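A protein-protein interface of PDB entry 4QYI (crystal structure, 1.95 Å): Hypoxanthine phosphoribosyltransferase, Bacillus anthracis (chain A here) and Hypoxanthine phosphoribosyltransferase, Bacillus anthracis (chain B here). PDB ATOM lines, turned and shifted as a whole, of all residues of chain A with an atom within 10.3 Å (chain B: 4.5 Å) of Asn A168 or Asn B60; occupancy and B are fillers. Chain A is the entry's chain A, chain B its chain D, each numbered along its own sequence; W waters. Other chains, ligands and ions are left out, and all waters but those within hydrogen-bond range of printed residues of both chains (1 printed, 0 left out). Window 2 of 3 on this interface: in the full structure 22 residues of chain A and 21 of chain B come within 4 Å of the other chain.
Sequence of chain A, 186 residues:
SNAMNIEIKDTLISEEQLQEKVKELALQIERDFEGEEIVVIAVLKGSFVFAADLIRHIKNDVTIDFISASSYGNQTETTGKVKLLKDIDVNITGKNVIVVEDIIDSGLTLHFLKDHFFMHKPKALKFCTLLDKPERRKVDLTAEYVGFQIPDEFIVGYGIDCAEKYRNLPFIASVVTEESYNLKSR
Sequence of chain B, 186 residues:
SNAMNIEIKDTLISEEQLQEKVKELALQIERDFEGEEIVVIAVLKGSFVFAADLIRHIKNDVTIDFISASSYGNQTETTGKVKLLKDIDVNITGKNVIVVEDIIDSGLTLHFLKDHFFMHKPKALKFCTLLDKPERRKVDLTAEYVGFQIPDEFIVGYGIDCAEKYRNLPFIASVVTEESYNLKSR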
ATOM      1  N   ILE A   8       0.772 -16.246 -27.299  1.00  0.00           N
ATOM      2  CA  ILE A   8      -0.366 -16.182 -26.406  1.00  0.00           C
ATOM      3  C   ILE A   8      -1.647 -16.365 -27.175  1.00  0.00           C
ATOM      4  O   ILE A   8      -1.795 -15.845 -28.268  1.00  0.00           O
ATOM      5  CB  ILE A   8      -0.378 -14.855 -25.650  1.00  0.00           C
ATOM      6  CG1 ILE A   8       0.951 -14.803 -24.853  1.00  0.00           C
ATOM      7  CG2 ILE A   8      -1.657 -14.721 -24.816  1.00  0.00           C
ATOM      8  CD1 ILE A   8       1.089 -13.759 -23.766  1.00  0.00           C
ATOM      9  N   GLU A  15      -6.415  -9.554 -14.906  1.00  0.00           N
ATOM     10  CA  GLU A  15      -5.706  -8.852 -13.867  1.00  0.00           C
ATOM     11  C   GLU A  15      -6.656  -8.549 -12.698  1.00  0.00           C
ATOM     12  O   GLU A  15      -6.332  -8.794 -11.538  1.00  0.00           O
ATOM     13  CB  GLU A  15      -5.150  -7.559 -14.465  1.00  0.00           C
ATOM     14  CG  GLU A  15      -4.418  -6.660 -13.493  1.00  0.00           C
ATOM     15  CD  GLU A  15      -3.812  -5.445 -14.183  1.00  0.00           C
ATOM     16  OE1 GLU A  15      -3.870  -5.341 -15.431  1.00  0.00           O
ATOM     17  OE2 GLU A  15      -3.243  -4.600 -13.472  1.00  0.00           O
ATOM     18  N   LEU A  18      -7.678 -11.629 -10.727  1.00  0.00           N
ATOM     19  CA  LEU A  18      -6.577 -12.059  -9.880  1.00  0.00           C
ATOM     20  C   LEU A  18      -6.529 -11.220  -8.624  1.00  0.00           C
ATOM     21  O   LEU A  18      -6.435 -11.767  -7.535  1.00  0.00           O
ATOM     22  CB  LEU A  18      -5.250 -11.964 -10.614  1.00  0.00           C
ATOM     23  CG  LEU A  18      -5.079 -13.001 -11.706  1.00  0.00           C
ATOM     24  CD1 LEU A  18      -3.941 -12.666 -12.657  1.00  0.00           C
ATOM     25  CD2 LEU A  18      -4.854 -14.342 -11.041  1.00  0.00           C
ATOM     26  N   LYS A  45      10.425 -20.310  -8.747  1.00  0.00           N
ATOM     27  CA  LYS A  45      10.370 -18.863  -8.947  1.00  0.00           C
ATOM     28  C   LYS A  45       8.960 -18.361  -9.178  1.00  0.00           C
ATOM     29  O   LYS A  45       8.643 -17.225  -8.840  1.00  0.00           O
ATOM     30  CB  LYS A  45      11.156 -18.498 -10.205  1.00  0.00           C
ATOM     31  CG  LYS A  45      12.636 -18.809 -10.123  1.00  0.00           C
ATOM     32  CD  LYS A  45      13.374 -18.638 -11.453  1.00  0.00           C
ATOM     33  CE  LYS A  45      14.820 -19.081 -11.274  1.00  0.00           C
ATOM     34  NZ  LYS A  45      15.617 -18.932 -12.512  1.00  0.00           N
ATOM     35  N   GLY A  46       8.110 -19.240  -9.694  1.00  0.00           N
ATOM     36  CA  GLY A  46       6.768 -18.891 -10.119  1.00  0.00           C
ATOM     37  C   GLY A  46       5.741 -18.308  -9.181  1.00  0.00           C
ATOM     38  O   GLY A  46       4.778 -17.695  -9.625  1.00  0.00           O
ATOM     39  N   PHE A  48       6.427 -15.995  -6.905  1.00  0.00           N
ATOM     40  CA  PHE A  48       6.852 -14.698  -6.335  1.00  0.00           C
ATOM     41  C   PHE A  48       5.896 -13.540  -6.537  1.00  0.00           C
ATOM     42  O   PHE A  48       5.793 -12.704  -5.651  1.00  0.00           O
ATOM     43  CB  PHE A  48       8.292 -14.292  -6.718  1.00  0.00           C
ATOM     44  CG  PHE A  48       8.430 -13.481  -7.980  1.00  0.00           C
ATOM     45  CD1 PHE A  48       8.408 -14.073  -9.234  1.00  0.00           C
ATOM     46  CD2 PHE A  48       8.643 -12.106  -7.901  1.00  0.00           C
ATOM     47  CE1 PHE A  48       8.551 -13.312 -10.381  1.00  0.00           C
ATOM     48  CE2 PHE A  48       8.798 -11.345  -9.044  1.00  0.00           C
ATOM     49  CZ  PHE A  48       8.764 -11.955 -10.284  1.00  0.00           C
ATOM     50  N   VAL A  49       5.175 -13.504  -7.652  1.00  0.00           N
ATOM     51  CA  VAL A  49       4.236 -12.403  -7.903  1.00  0.00           C
ATOM     52  C   VAL A  49       3.020 -12.580  -7.011  1.00  0.00           C
ATOM     53  O   VAL A  49       2.591 -11.663  -6.336  1.00  0.00           O
ATOM     54  CB  VAL A  49       3.835 -12.318  -9.388  1.00  0.00           C
ATOM     55  CG1 VAL A  49       2.786 -11.248  -9.585  1.00  0.00           C
ATOM     56  CG2 VAL A  49       5.055 -12.038 -10.257  1.00  0.00           C
ATOM     57  N   VAL A 156       0.516 -19.165 -18.771  1.00  0.00           N
ATOM     58  CA  VAL A 156       1.620 -18.264 -18.488  1.00  0.00           C
ATOM     59  C   VAL A 156       1.067 -16.988 -17.888  1.00  0.00           C
ATOM     60  O   VAL A 156      -0.148 -16.752 -17.923  1.00  0.00           O
ATOM     61  CB  VAL A 156       2.425 -17.901 -19.765  1.00  0.00           C
ATOM     62  CG1 VAL A 156       3.065 -19.141 -20.379  1.00  0.00           C
ATOM     63  CG2 VAL A 156       1.546 -17.195 -20.784  1.00  0.00           C
ATOM     64  N   GLY A 157       1.961 -16.175 -17.333  1.00  0.00           N
ATOM     65  CA  GLY A 157       1.598 -14.894 -16.725  1.00  0.00           C
ATOM     66  C   GLY A 157       1.580 -14.876 -15.200  1.00  0.00           C
ATOM     67  O   GLY A 157       1.562 -15.927 -14.547  1.00  0.00           O
ATOM     68  N   TYR A 158       1.603 -13.671 -14.630  1.00  0.00           N
ATOM     69  CA  TYR A 158       1.520 -13.495 -13.184  1.00  0.00           C
ATOM     70  C   TYR A 158       2.548 -14.387 -12.450  1.00  0.00           C
ATOM     71  O   TYR A 158       2.217 -15.095 -11.503  1.00  0.00           O
ATOM     72  CB  TYR A 158       0.070 -13.785 -12.732  1.00  0.00           C
ATOM     73  CG  TYR A 158      -0.307 -13.249 -11.362  1.00  0.00           C
ATOM     74  CD1 TYR A 158      -0.609 -11.895 -11.172  1.00  0.00           C
ATOM     75  CD2 TYR A 158      -0.416 -14.097 -10.267  1.00  0.00           C
ATOM     76  CE1 TYR A 158      -0.957 -11.406  -9.922  1.00  0.00           C
ATOM     77  CE2 TYR A 158      -0.781 -13.618  -9.015  1.00  0.00           C
ATOM     78  CZ  TYR A 158      -1.052 -12.277  -8.853  1.00  0.00           C
ATOM     79  OH  TYR A 158      -1.390 -11.827  -7.599  1.00  0.00           O
ATOM     80  N   GLY A 159       3.795 -14.326 -12.909  1.00  0.00           N
ATOM     81  CA  GLY A 159       4.884 -15.113 -12.335  1.00  0.00           C
ATOM     82  C   GLY A 159       5.195 -16.457 -12.970  1.00  0.00           C
ATOM     83  O   GLY A 159       6.306 -16.958 -12.839  1.00  0.00           O
ATOM     84  N   ILE A 160       4.230 -17.007 -13.704  1.00  0.00           N
ATOM     85  CA  ILE A 160       4.349 -18.300 -14.373  1.00  0.00           C
ATOM     86  C   ILE A 160       4.916 -18.139 -15.785  1.00  0.00           C
ATOM     87  O   ILE A 160       4.429 -17.336 -16.606  1.00  0.00           O
ATOM     88  CB  ILE A 160       2.960 -18.960 -14.456  1.00  0.00           C
ATOM     89  CG1 ILE A 160       2.330 -18.951 -13.073  1.00  0.00           C
ATOM     90  CG2 ILE A 160       3.035 -20.380 -15.006  1.00  0.00           C
ATOM     91  CD1 ILE A 160       0.877 -19.359 -13.039  1.00  0.00           C
ATOM     92  N   ASP A 161       5.923 -18.940 -16.103  1.00  0.00           N
ATOM     93  CA  ASP A 161       6.570 -18.858 -17.406  1.00  0.00           C
ATOM     94  C   ASP A 161       6.351 -20.043 -18.330  1.00  0.00           C
ATOM     95  O   ASP A 161       5.728 -21.039 -17.994  1.00  0.00           O
ATOM     96  CB  ASP A 161       8.082 -18.845 -17.221  1.00  0.00           C
ATOM     97  CG  ASP A 161       8.622 -20.209 -16.776  1.00  0.00           C
ATOM     98  OD1 ASP A 161       8.092 -20.785 -15.806  1.00  0.00           O
ATOM     99  OD2 ASP A 161       9.584 -20.717 -17.393  1.00  0.00           O
ATOM    100  N   CYS A 162       6.874 -19.872 -19.532  1.00  0.00           N
ATOM    101  CA  CYS A 162       6.961 -20.928 -20.522  1.00  0.00           C
ATOM    102  C   CYS A 162       8.368 -20.641 -21.054  1.00  0.00           C
ATOM    103  O   CYS A 162       8.619 -19.610 -21.695  1.00  0.00           O
ATOM    104  CB  CYS A 162       5.893 -20.850 -21.596  1.00  0.00           C
ATOM    105  SG  CYS A 162       6.312 -21.971 -22.951  1.00  0.00           S
ATOM    106  N   GLU A 164      10.917 -19.639 -19.407  1.00  0.00           N
ATOM    107  CA  GLU A 164      11.359 -18.383 -18.774  1.00  0.00           C
ATOM    108  C   GLU A 164      10.715 -17.112 -19.360  1.00  0.00           C
ATOM    109  O   GLU A 164      11.077 -15.998 -18.983  1.00  0.00           O
ATOM    110  CB  GLU A 164      12.900 -18.269 -18.775  1.00  0.00           C
ATOM    111  CG  GLU A 164      13.622 -19.415 -18.064  1.00  0.00           C
ATOM    112  CD  GLU A 164      13.232 -19.572 -16.595  1.00  0.00           C
ATOM    113  OE1 GLU A 164      12.750 -18.607 -15.964  1.00  0.00           O
ATOM    114  OE2 GLU A 164      13.407 -20.681 -16.055  1.00  0.00           O
ATOM    115  N   LYS A 165       9.767 -17.287 -20.277  1.00  0.00           N
ATOM    116  CA  LYS A 165       9.082 -16.172 -20.920  1.00  0.00           C
ATOM    117  C   LYS A 165       7.680 -15.959 -20.329  1.00  0.00           C
ATOM    118  O   LYS A 165       7.093 -16.870 -19.735  1.00  0.00           O
ATOM    119  CB  LYS A 165       9.045 -16.443 -22.438  1.00  0.00           C
ATOM    120  CG  LYS A 165       8.395 -15.385 -23.320  1.00  0.00           C
ATOM    121  CD  LYS A 165       8.488 -15.772 -24.794  1.00  0.00           C
ATOM    122  CE  LYS A 165       7.922 -14.693 -25.715  1.00  0.00           C
ATOM    123  NZ  LYS A 165       8.688 -13.417 -25.749  1.00  0.00           N
ATOM    124  N   TYR A 166       7.208 -14.716 -20.406  1.00  0.00           N
ATOM    125  CA  TYR A 166       5.867 -14.311 -19.966  1.00  0.00           C
ATOM    126  C   TYR A 166       5.555 -14.181 -18.467  1.00  0.00           C
ATOM    127  O   TYR A 166       4.401 -13.974 -18.108  1.00  0.00           O
ATOM    128  CB  TYR A 166       4.803 -15.200 -20.614  1.00  0.00           C
ATOM    129  CG  TYR A 166       4.813 -15.171 -22.125  1.00  0.00           C
ATOM    130  CD1 TYR A 166       4.594 -13.983 -22.814  1.00  0.00           C
ATOM    131  CD2 TYR A 166       4.981 -16.335 -22.860  1.00  0.00           C
ATOM    132  CE1 TYR A 166       4.588 -13.953 -24.196  1.00  0.00           C
ATOM    133  CE2 TYR A 166       4.969 -16.320 -24.242  1.00  0.00           C
ATOM    134  CZ  TYR A 166       4.765 -15.128 -24.908  1.00  0.00           C
ATOM    135  OH  TYR A 166       4.765 -15.125 -26.290  1.00  0.00           O
ATOM    136  N   ARG A 167       6.547 -14.262 -17.589  1.00  0.00           N
ATOM    137  CA  ARG A 167       6.266 -14.119 -16.149  1.00  0.00           C
ATOM    138  C   ARG A 167       5.743 -12.739 -15.813  1.00  0.00           C
ATOM    139  O   ARG A 167       5.105 -12.559 -14.780  1.00  0.00           O
ATOM    140  CB  ARG A 167       7.516 -14.345 -15.294  1.00  0.00           C
ATOM    141  CG  ARG A 167       8.113 -15.734 -15.365  1.00  0.00           C
ATOM    142  CD  ARG A 167       9.120 -15.900 -14.241  1.00  0.00           C
ATOM    143  NE  ARG A 167       9.933 -17.100 -14.371  1.00  0.00           N
ATOM    144  CZ  ARG A 167       9.614 -18.306 -13.916  1.00  0.00           C
ATOM    145  NH1 ARG A 167       8.471 -18.531 -13.281  1.00  0.00           N
ATOM    146  NH2 ARG A 167      10.459 -19.300 -14.105  1.00  0.00           N
ATOM    147  N   ASN A 168       6.004 -11.767 -16.686  1.00  0.00           N
ATOM    148  CA  ASN A 168       5.617 -10.402 -16.413  1.00  0.00           C
ATOM    149  C   ASN A 168       4.222  -9.981 -16.857  1.00  0.00           C
ATOM    150  O   ASN A 168       3.861  -8.828 -16.671  1.00  0.00           O
ATOM    151  CB  ASN A 168       6.628  -9.444 -17.017  1.00  0.00           C
ATOM    152  CG  ASN A 168       6.677  -9.533 -18.516  1.00  0.00           C
ATOM    153  OD1 ASN A 168       6.552 -10.609 -19.095  1.00  0.00           O
ATOM    154  ND2 ASN A 168       6.846  -8.395 -19.157  1.00  0.00           N
ATOM    155  N   LEU A 169       3.432 -10.891 -17.419  1.00  0.00           N
ATOM    156  CA  LEU A 169       2.070 -10.521 -17.771  1.00  0.00           C
ATOM    157  C   LEU A 169       1.270 -10.283 -16.490  1.00  0.00           C
ATOM    158  O   LEU A 169       1.409 -11.030 -15.533  1.00  0.00           O
ATOM    159  CB  LEU A 169       1.383 -11.619 -18.577  1.00  0.00           C
ATOM    160  CG  LEU A 169       2.094 -12.061 -19.850  1.00  0.00           C
ATOM    161  CD1 LEU A 169       1.285 -13.139 -20.550  1.00  0.00           C
ATOM    162  CD2 LEU A 169       2.329 -10.890 -20.793  1.00  0.00           C
ATOM    163  N   PRO A 170       0.423  -9.240 -16.459  1.00  0.00           N
ATOM    164  CA  PRO A 170      -0.373  -8.992 -15.257  1.00  0.00           C
ATOM    165  C   PRO A 170      -1.631  -9.854 -15.149  1.00  0.00           C
ATOM    166  O   PRO A 170      -2.386  -9.745 -14.174  1.00  0.00           O
ATOM    167  CB  PRO A 170      -0.739  -7.521 -15.390  1.00  0.00           C
ATOM    168  CG  PRO A 170      -0.776  -7.277 -16.865  1.00  0.00           C
ATOM    169  CD  PRO A 170       0.328  -8.130 -17.428  1.00  0.00           C
ATOM    170  N   PHE A 171      -1.833 -10.717 -16.141  1.00  0.00           N
ATOM    171  CA  PHE A 171      -2.973 -11.625 -16.210  1.00  0.00           C
ATOM    172  C   PHE A 171      -2.435 -13.016 -16.539  1.00  0.00           C
ATOM    173  O   PHE A 171      -1.246 -13.169 -16.831  1.00  0.00           O
ATOM    174  CB  PHE A 171      -3.942 -11.162 -17.326  1.00  0.00           C
ATOM    175  CG  PHE A 171      -3.266 -10.978 -18.653  1.00  0.00           C
ATOM    176  CD1 PHE A 171      -3.070 -12.056 -19.513  1.00  0.00           C
ATOM    177  CD2 PHE A 171      -2.802  -9.727 -19.036  1.00  0.00           C
ATOM    178  CE1 PHE A 171      -2.421 -11.890 -20.730  1.00  0.00           C
ATOM    179  CE2 PHE A 171      -2.175  -9.545 -20.254  1.00  0.00           C
ATOM    180  CZ  PHE A 171      -1.974 -10.625 -21.099  1.00  0.00           C
ATOM    181  N   ILE A 172      -3.310 -14.017 -16.485  1.00  0.00           N
ATOM    182  CA  ILE A 172      -2.966 -15.390 -16.827  1.00  0.00           C
ATOM    183  C   ILE A 172      -3.592 -15.717 -18.183  1.00  0.00           C
ATOM    184  O   ILE A 172      -4.771 -15.449 -18.421  1.00  0.00           O
ATOM    185  CB  ILE A 172      -3.395 -16.375 -15.732  1.00  0.00           C
ATOM    186  CG1 ILE A 172      -2.514 -16.099 -14.483  1.00  0.00           C
ATOM    187  CG2 ILE A 172      -3.246 -17.816 -16.198  1.00  0.00           C
ATOM    188  CD1 ILE A 172      -2.548 -17.089 -13.354  1.00  0.00           C
ATOM    189  N   ALA A 173      -2.787 -16.295 -19.074  1.00  0.00           N
ATOM    190  CA  ALA A 173      -3.238 -16.628 -20.416  1.00  0.00           C
ATOM    191  C   ALA A 173      -2.870 -18.019 -20.872  1.00  0.00           C
ATOM    192  O   ALA A 173      -1.935 -18.621 -20.361  1.00  0.00           O
ATOM    193  CB  ALA A 173      -2.635 -15.641 -21.399  1.00  0.00           C
ATOM    194  N   GLU B  30      11.262   1.248 -20.374  1.00  0.00           N
ATOM    195  CA  GLU B  30      10.734   0.971 -21.708  1.00  0.00           C
ATOM    196  C   GLU B  30      11.327   1.914 -22.757  1.00  0.00           C
ATOM    197  O   GLU B  30      11.659   1.493 -23.859  1.00  0.00           O
ATOM    198  CB  GLU B  30       9.214   1.123 -21.740  1.00  0.00           C
ATOM    199  CG  GLU B  30       8.450   0.049 -20.987  1.00  0.00           C
ATOM    200  CD  GLU B  30       6.947   0.280 -21.023  1.00  0.00           C
ATOM    201  OE1 GLU B  30       6.515   1.461 -20.890  1.00  0.00           O
ATOM    202  OE2 GLU B  30       6.192  -0.708 -21.177  1.00  0.00           O
ATOM    203  N   PHE B  33      14.946   0.970 -23.765  1.00  0.00           N
ATOM    204  CA  PHE B  33      15.144  -0.308 -24.434  1.00  0.00           C
ATOM    205  C   PHE B  33      14.011  -0.612 -25.408  1.00  0.00           C
ATOM    206  O   PHE B  33      13.525  -1.736 -25.507  1.00  0.00           O
ATOM    207  CB  PHE B  33      15.285  -1.432 -23.373  1.00  0.00           C
ATOM    208  CG  PHE B  33      16.466  -1.248 -22.447  1.00  0.00           C
ATOM    209  CD1 PHE B  33      17.740  -1.648 -22.831  1.00  0.00           C
ATOM    210  CD2 PHE B  33      16.308  -0.668 -21.201  1.00  0.00           C
ATOM    211  CE1 PHE B  33      18.838  -1.464 -22.004  1.00  0.00           C
ATOM    212  CE2 PHE B  33      17.403  -0.507 -20.349  1.00  0.00           C
ATOM    213  CZ  PHE B  33      18.671  -0.896 -20.756  1.00  0.00           C
ATOM    214  N   GLY B  35      11.815  -1.771 -28.268  1.00  0.00           N
ATOM    215  CA  GLY B  35      11.919  -2.893 -29.206  1.00  0.00           C
ATOM    216  C   GLY B  35      12.869  -4.024 -28.835  1.00  0.00           C
ATOM    217  O   GLY B  35      13.164  -4.885 -29.666  1.00  0.00           O
ATOM    218  N   GLU B  36      13.335  -4.070 -27.595  1.00  0.00           N
ATOM    219  CA  GLU B  36      14.292  -5.110 -27.249  1.00  0.00           C
ATOM    220  C   GLU B  36      13.960  -5.836 -25.936  1.00  0.00           C
ATOM    221  O   GLU B  36      13.172  -5.346 -25.109  1.00  0.00           O
ATOM    222  CB  GLU B  36      15.727  -4.522 -27.388  1.00  0.00           C
ATOM    223  CG  GLU B  36      15.906  -3.114 -26.822  1.00  0.00           C
ATOM    224  CD  GLU B  36      17.205  -2.446 -27.236  1.00  0.00           C
ATOM    225  OE1 GLU B  36      17.703  -2.689 -28.352  1.00  0.00           O
ATOM    226  OE2 GLU B  36      17.718  -1.637 -26.442  1.00  0.00           O
ATOM    227  N   ILE B  38      14.634  -7.674 -22.311  1.00  0.00           N
ATOM    228  CA  ILE B  38      15.340  -7.240 -21.127  1.00  0.00           C
ATOM    229  C   ILE B  38      15.392  -8.370 -20.128  1.00  0.00           C
ATOM    230  O   ILE B  38      14.448  -9.161 -20.041  1.00  0.00           O
ATOM    231  CB  ILE B  38      14.597  -6.103 -20.409  1.00  0.00           C
ATOM    232  CG1 ILE B  38      14.461  -4.893 -21.326  1.00  0.00           C
ATOM    233  CG2 ILE B  38      15.348  -5.688 -19.151  1.00  0.00           C
ATOM    234  CD1 ILE B  38      13.511  -3.848 -20.775  1.00  0.00           C
ATOM    235  N   ILE B  55       7.999  -5.120 -13.100  1.00  0.00           N
ATOM    236  CA  ILE B  55       7.941  -5.876 -14.349  1.00  0.00           C
ATOM    237  C   ILE B  55       6.560  -5.934 -14.982  1.00  0.00           C
ATOM    238  O   ILE B  55       6.444  -6.030 -16.208  1.00  0.00           O
ATOM    239  CB  ILE B  55       8.558  -7.273 -14.232  1.00  0.00           C
ATOM    240  CG1 ILE B  55       7.706  -8.201 -13.363  1.00  0.00           C
ATOM    241  CG2 ILE B  55       9.991  -7.149 -13.726  1.00  0.00           C
ATOM    242  CD1 ILE B  55       8.243  -9.613 -13.305  1.00  0.00           C
ATOM    243  N   ARG B  56       5.519  -5.840 -14.162  1.00  0.00           N
ATOM    244  CA  ARG B  56       4.151  -5.879 -14.671  1.00  0.00           C
ATOM    245  C   ARG B  56       3.763  -4.637 -15.457  1.00  0.00           C
ATOM    246  O   ARG B  56       2.751  -4.635 -16.127  1.00  0.00           O
ATOM    247  CB  ARG B  56       3.156  -6.188 -13.552  1.00  0.00           C
ATOM    248  CG  ARG B  56       3.187  -7.664 -13.192  1.00  0.00           C
ATOM    249  CD  ARG B  56       2.165  -8.023 -12.134  1.00  0.00           C
ATOM    250  NE  ARG B  56       2.608  -7.582 -10.818  1.00  0.00           N
ATOM    251  CZ  ARG B  56       1.932  -7.757  -9.694  1.00  0.00           C
ATOM    252  NH1 ARG B  56       0.751  -8.361  -9.716  1.00  0.00           N
ATOM    253  NH2 ARG B  56       2.444  -7.315  -8.547  1.00  0.00           N
ATOM    254  N   ILE B  58       6.183  -3.212 -17.417  1.00  0.00           N
ATOM    255  CA  ILE B  58       7.083  -3.235 -18.555  1.00  0.00           C
ATOM    256  C   ILE B  58       6.496  -4.137 -19.639  1.00  0.00           C
ATOM    257  O   ILE B  58       6.253  -5.330 -19.433  1.00  0.00           O
ATOM    258  CB  ILE B  58       8.489  -3.694 -18.158  1.00  0.00           C
ATOM    259  CG1 ILE B  58       9.122  -2.687 -17.185  1.00  0.00           C
ATOM    260  CG2 ILE B  58       9.370  -3.840 -19.395  1.00  0.00           C
ATOM    261  CD1 ILE B  58      10.400  -3.184 -16.531  1.00  0.00           C
ATOM    262  N   LYS B  59       6.283  -3.551 -20.814  1.00  0.00           N
ATOM    263  CA  LYS B  59       5.688  -4.250 -21.944  1.00  0.00           C
ATOM    264  C   LYS B  59       6.673  -5.084 -22.741  1.00  0.00           C
ATOM    265  O   LYS B  59       6.283  -6.015 -23.442  1.00  0.00           O
ATOM    266  CB  LYS B  59       5.032  -3.215 -22.862  1.00  0.00           C
ATOM    267  CG  LYS B  59       4.281  -3.816 -24.037  1.00  0.00           C
ATOM    268  CD  LYS B  59       3.659  -2.723 -24.915  1.00  0.00           C
ATOM    269  CE  LYS B  59       2.902  -3.257 -26.125  1.00  0.00           C
ATOM    270  NZ  LYS B  59       2.388  -2.148 -26.987  1.00  0.00           N
ATOM    271  N   ASN B  60       7.945  -4.727 -22.667  1.00  0.00           N
ATOM    272  CA  ASN B  60       8.970  -5.486 -23.373  1.00  0.00           C
ATOM    273  C   ASN B  60       8.967  -6.940 -22.922  1.00  0.00           C
ATOM    274  O   ASN B  60       8.415  -7.269 -21.871  1.00  0.00           O
ATOM    275  CB  ASN B  60      10.370  -4.958 -23.048  1.00  0.00           C
ATOM    276  CG  ASN B  60      10.542  -3.486 -23.366  1.00  0.00           C
ATOM    277  OD1 ASN B  60       9.820  -2.628 -22.857  1.00  0.00           O
ATOM    278  ND2 ASN B  60      11.556  -3.182 -24.160  1.00  0.00           N
ATOM    279  N   ASP B  61       9.577  -7.798 -23.730  1.00  0.00           N
ATOM    280  CA  ASP B  61       9.740  -9.186 -23.369  1.00  0.00           C
ATOM    281  C   ASP B  61      10.749  -9.193 -22.209  1.00  0.00           C
ATOM    282  O   ASP B  61      11.903  -8.790 -22.372  1.00  0.00           O
ATOM    283  CB  ASP B  61      10.248  -9.989 -24.555  1.00  0.00           C
ATOM    284  CG  ASP B  61      10.585 -11.421 -24.183  1.00  0.00           C
ATOM    285  OD1 ASP B  61      10.619 -11.743 -22.974  1.00  0.00           O
ATOM    286  OD2 ASP B  61      10.832 -12.229 -25.102  1.00  0.00           O
ATOM    287  N   VAL B  62      10.302  -9.622 -21.032  1.00  0.00           N
ATOM    288  CA  VAL B  62      11.152  -9.632 -19.860  1.00  0.00           C
ATOM    289  C   VAL B  62      11.424 -11.030 -19.334  1.00  0.00           C
ATOM    290  O   VAL B  62      10.524 -11.867 -19.257  1.00  0.00           O
ATOM    291  CB  VAL B  62      10.504  -8.829 -18.715  1.00  0.00           C
ATOM    292  CG1 VAL B  62      11.250  -9.039 -17.408  1.00  0.00           C
ATOM    293  CG2 VAL B  62      10.438  -7.352 -19.056  1.00  0.00           C
HETATM  294  O   HOH W   1       9.531 -13.817 -17.793  1.00  0.00           O
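Of the 24 printed residues of chain A, 5 touch a printed residue of chain B.
Hydrophobic or aromatic side chains of chain A that line the printed part of chain B: Phe A48, Val A49 and Tyr A158.
NZ of Lys A165 lies within salt-bridge range of OD2 of Asp B61 (2.5 Å).
ND2 of Asn A168 is in hydrogen-bond range of O of Ile B58.
ND2 of Asn A168 is in hydrogen-bond range of O of Asn B60 (3.3 Å).
CZ of Phe A48 touches CD1 of Ile B55 (3.9 Å).
CG1 of Val A49 touches NH1 of Arg B56 (3.5 Å).
CE1 of Tyr A158 touches NH1 of Arg B56 (3.5 Å).
Asn A168 touches Ile B55.
CA of Arg B56 touches O of Asn A168, 3.6 Å away.
Val B62 touches Asn A168.
Of the printed residues of chain A, Asn B60 touches Asn A168.
No residue of chain A comes within 4 Å of Glu B30.
Gly B35 touches none of the printed residues of chain A.
Ile B55 touches just these residues of chain A: Phe A48 and Asn A168.
Of the printed residues of chain A, Asp B61 touches Lys A165.
Val B62 touches just one residue of chain A: Asn A168 (3.7 Å).
Of the printed residues of chain A, Ile B58 touches Asn A168.
Printed residues of chain B within 4 Å of Phe A48: Ile B55.
Of the printed residues of chain B, Val A49 touches Arg B56 (3.5 Å).
Of the printed residues of chain A, Arg B56 touches Val A49 (3.5 Å), Tyr A158 (3.5 Å) and Asn A168 (3.6 Å).
Asp A161 touches none of the printed residues of chain B.
The nearest printed residue of chain B that does not touch Asn A168 is Lys B59 (4.9 Å).
Water W1 lies within hydrogen-bond range of O of Val B62 (2.6 Å), O of Glu A164 (2.9 Å) and N of Arg A167 (3.0 Å).
The backbone NH (N) of Tyr A158 lies within hydrogen-bond range of the backbone carbonyl oxygen (O) of Leu A169 (2.8 Å).
The backbone carbonyl oxygen (O) of Phe B33 lies within hydrogen-bond range of the side-chain amide nitrogen (ND2) of Asn B60.
The side-chain amide nitrogen of Asn B60 sits at hydrogen-bond distance from the backbone carbonyl oxygen of Glu B36 (2.9 Å).
The backbone NH (N) of Ile B38 is in hydrogen-bond range of the backbone carbonyl oxygen (O) of Asp B61.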
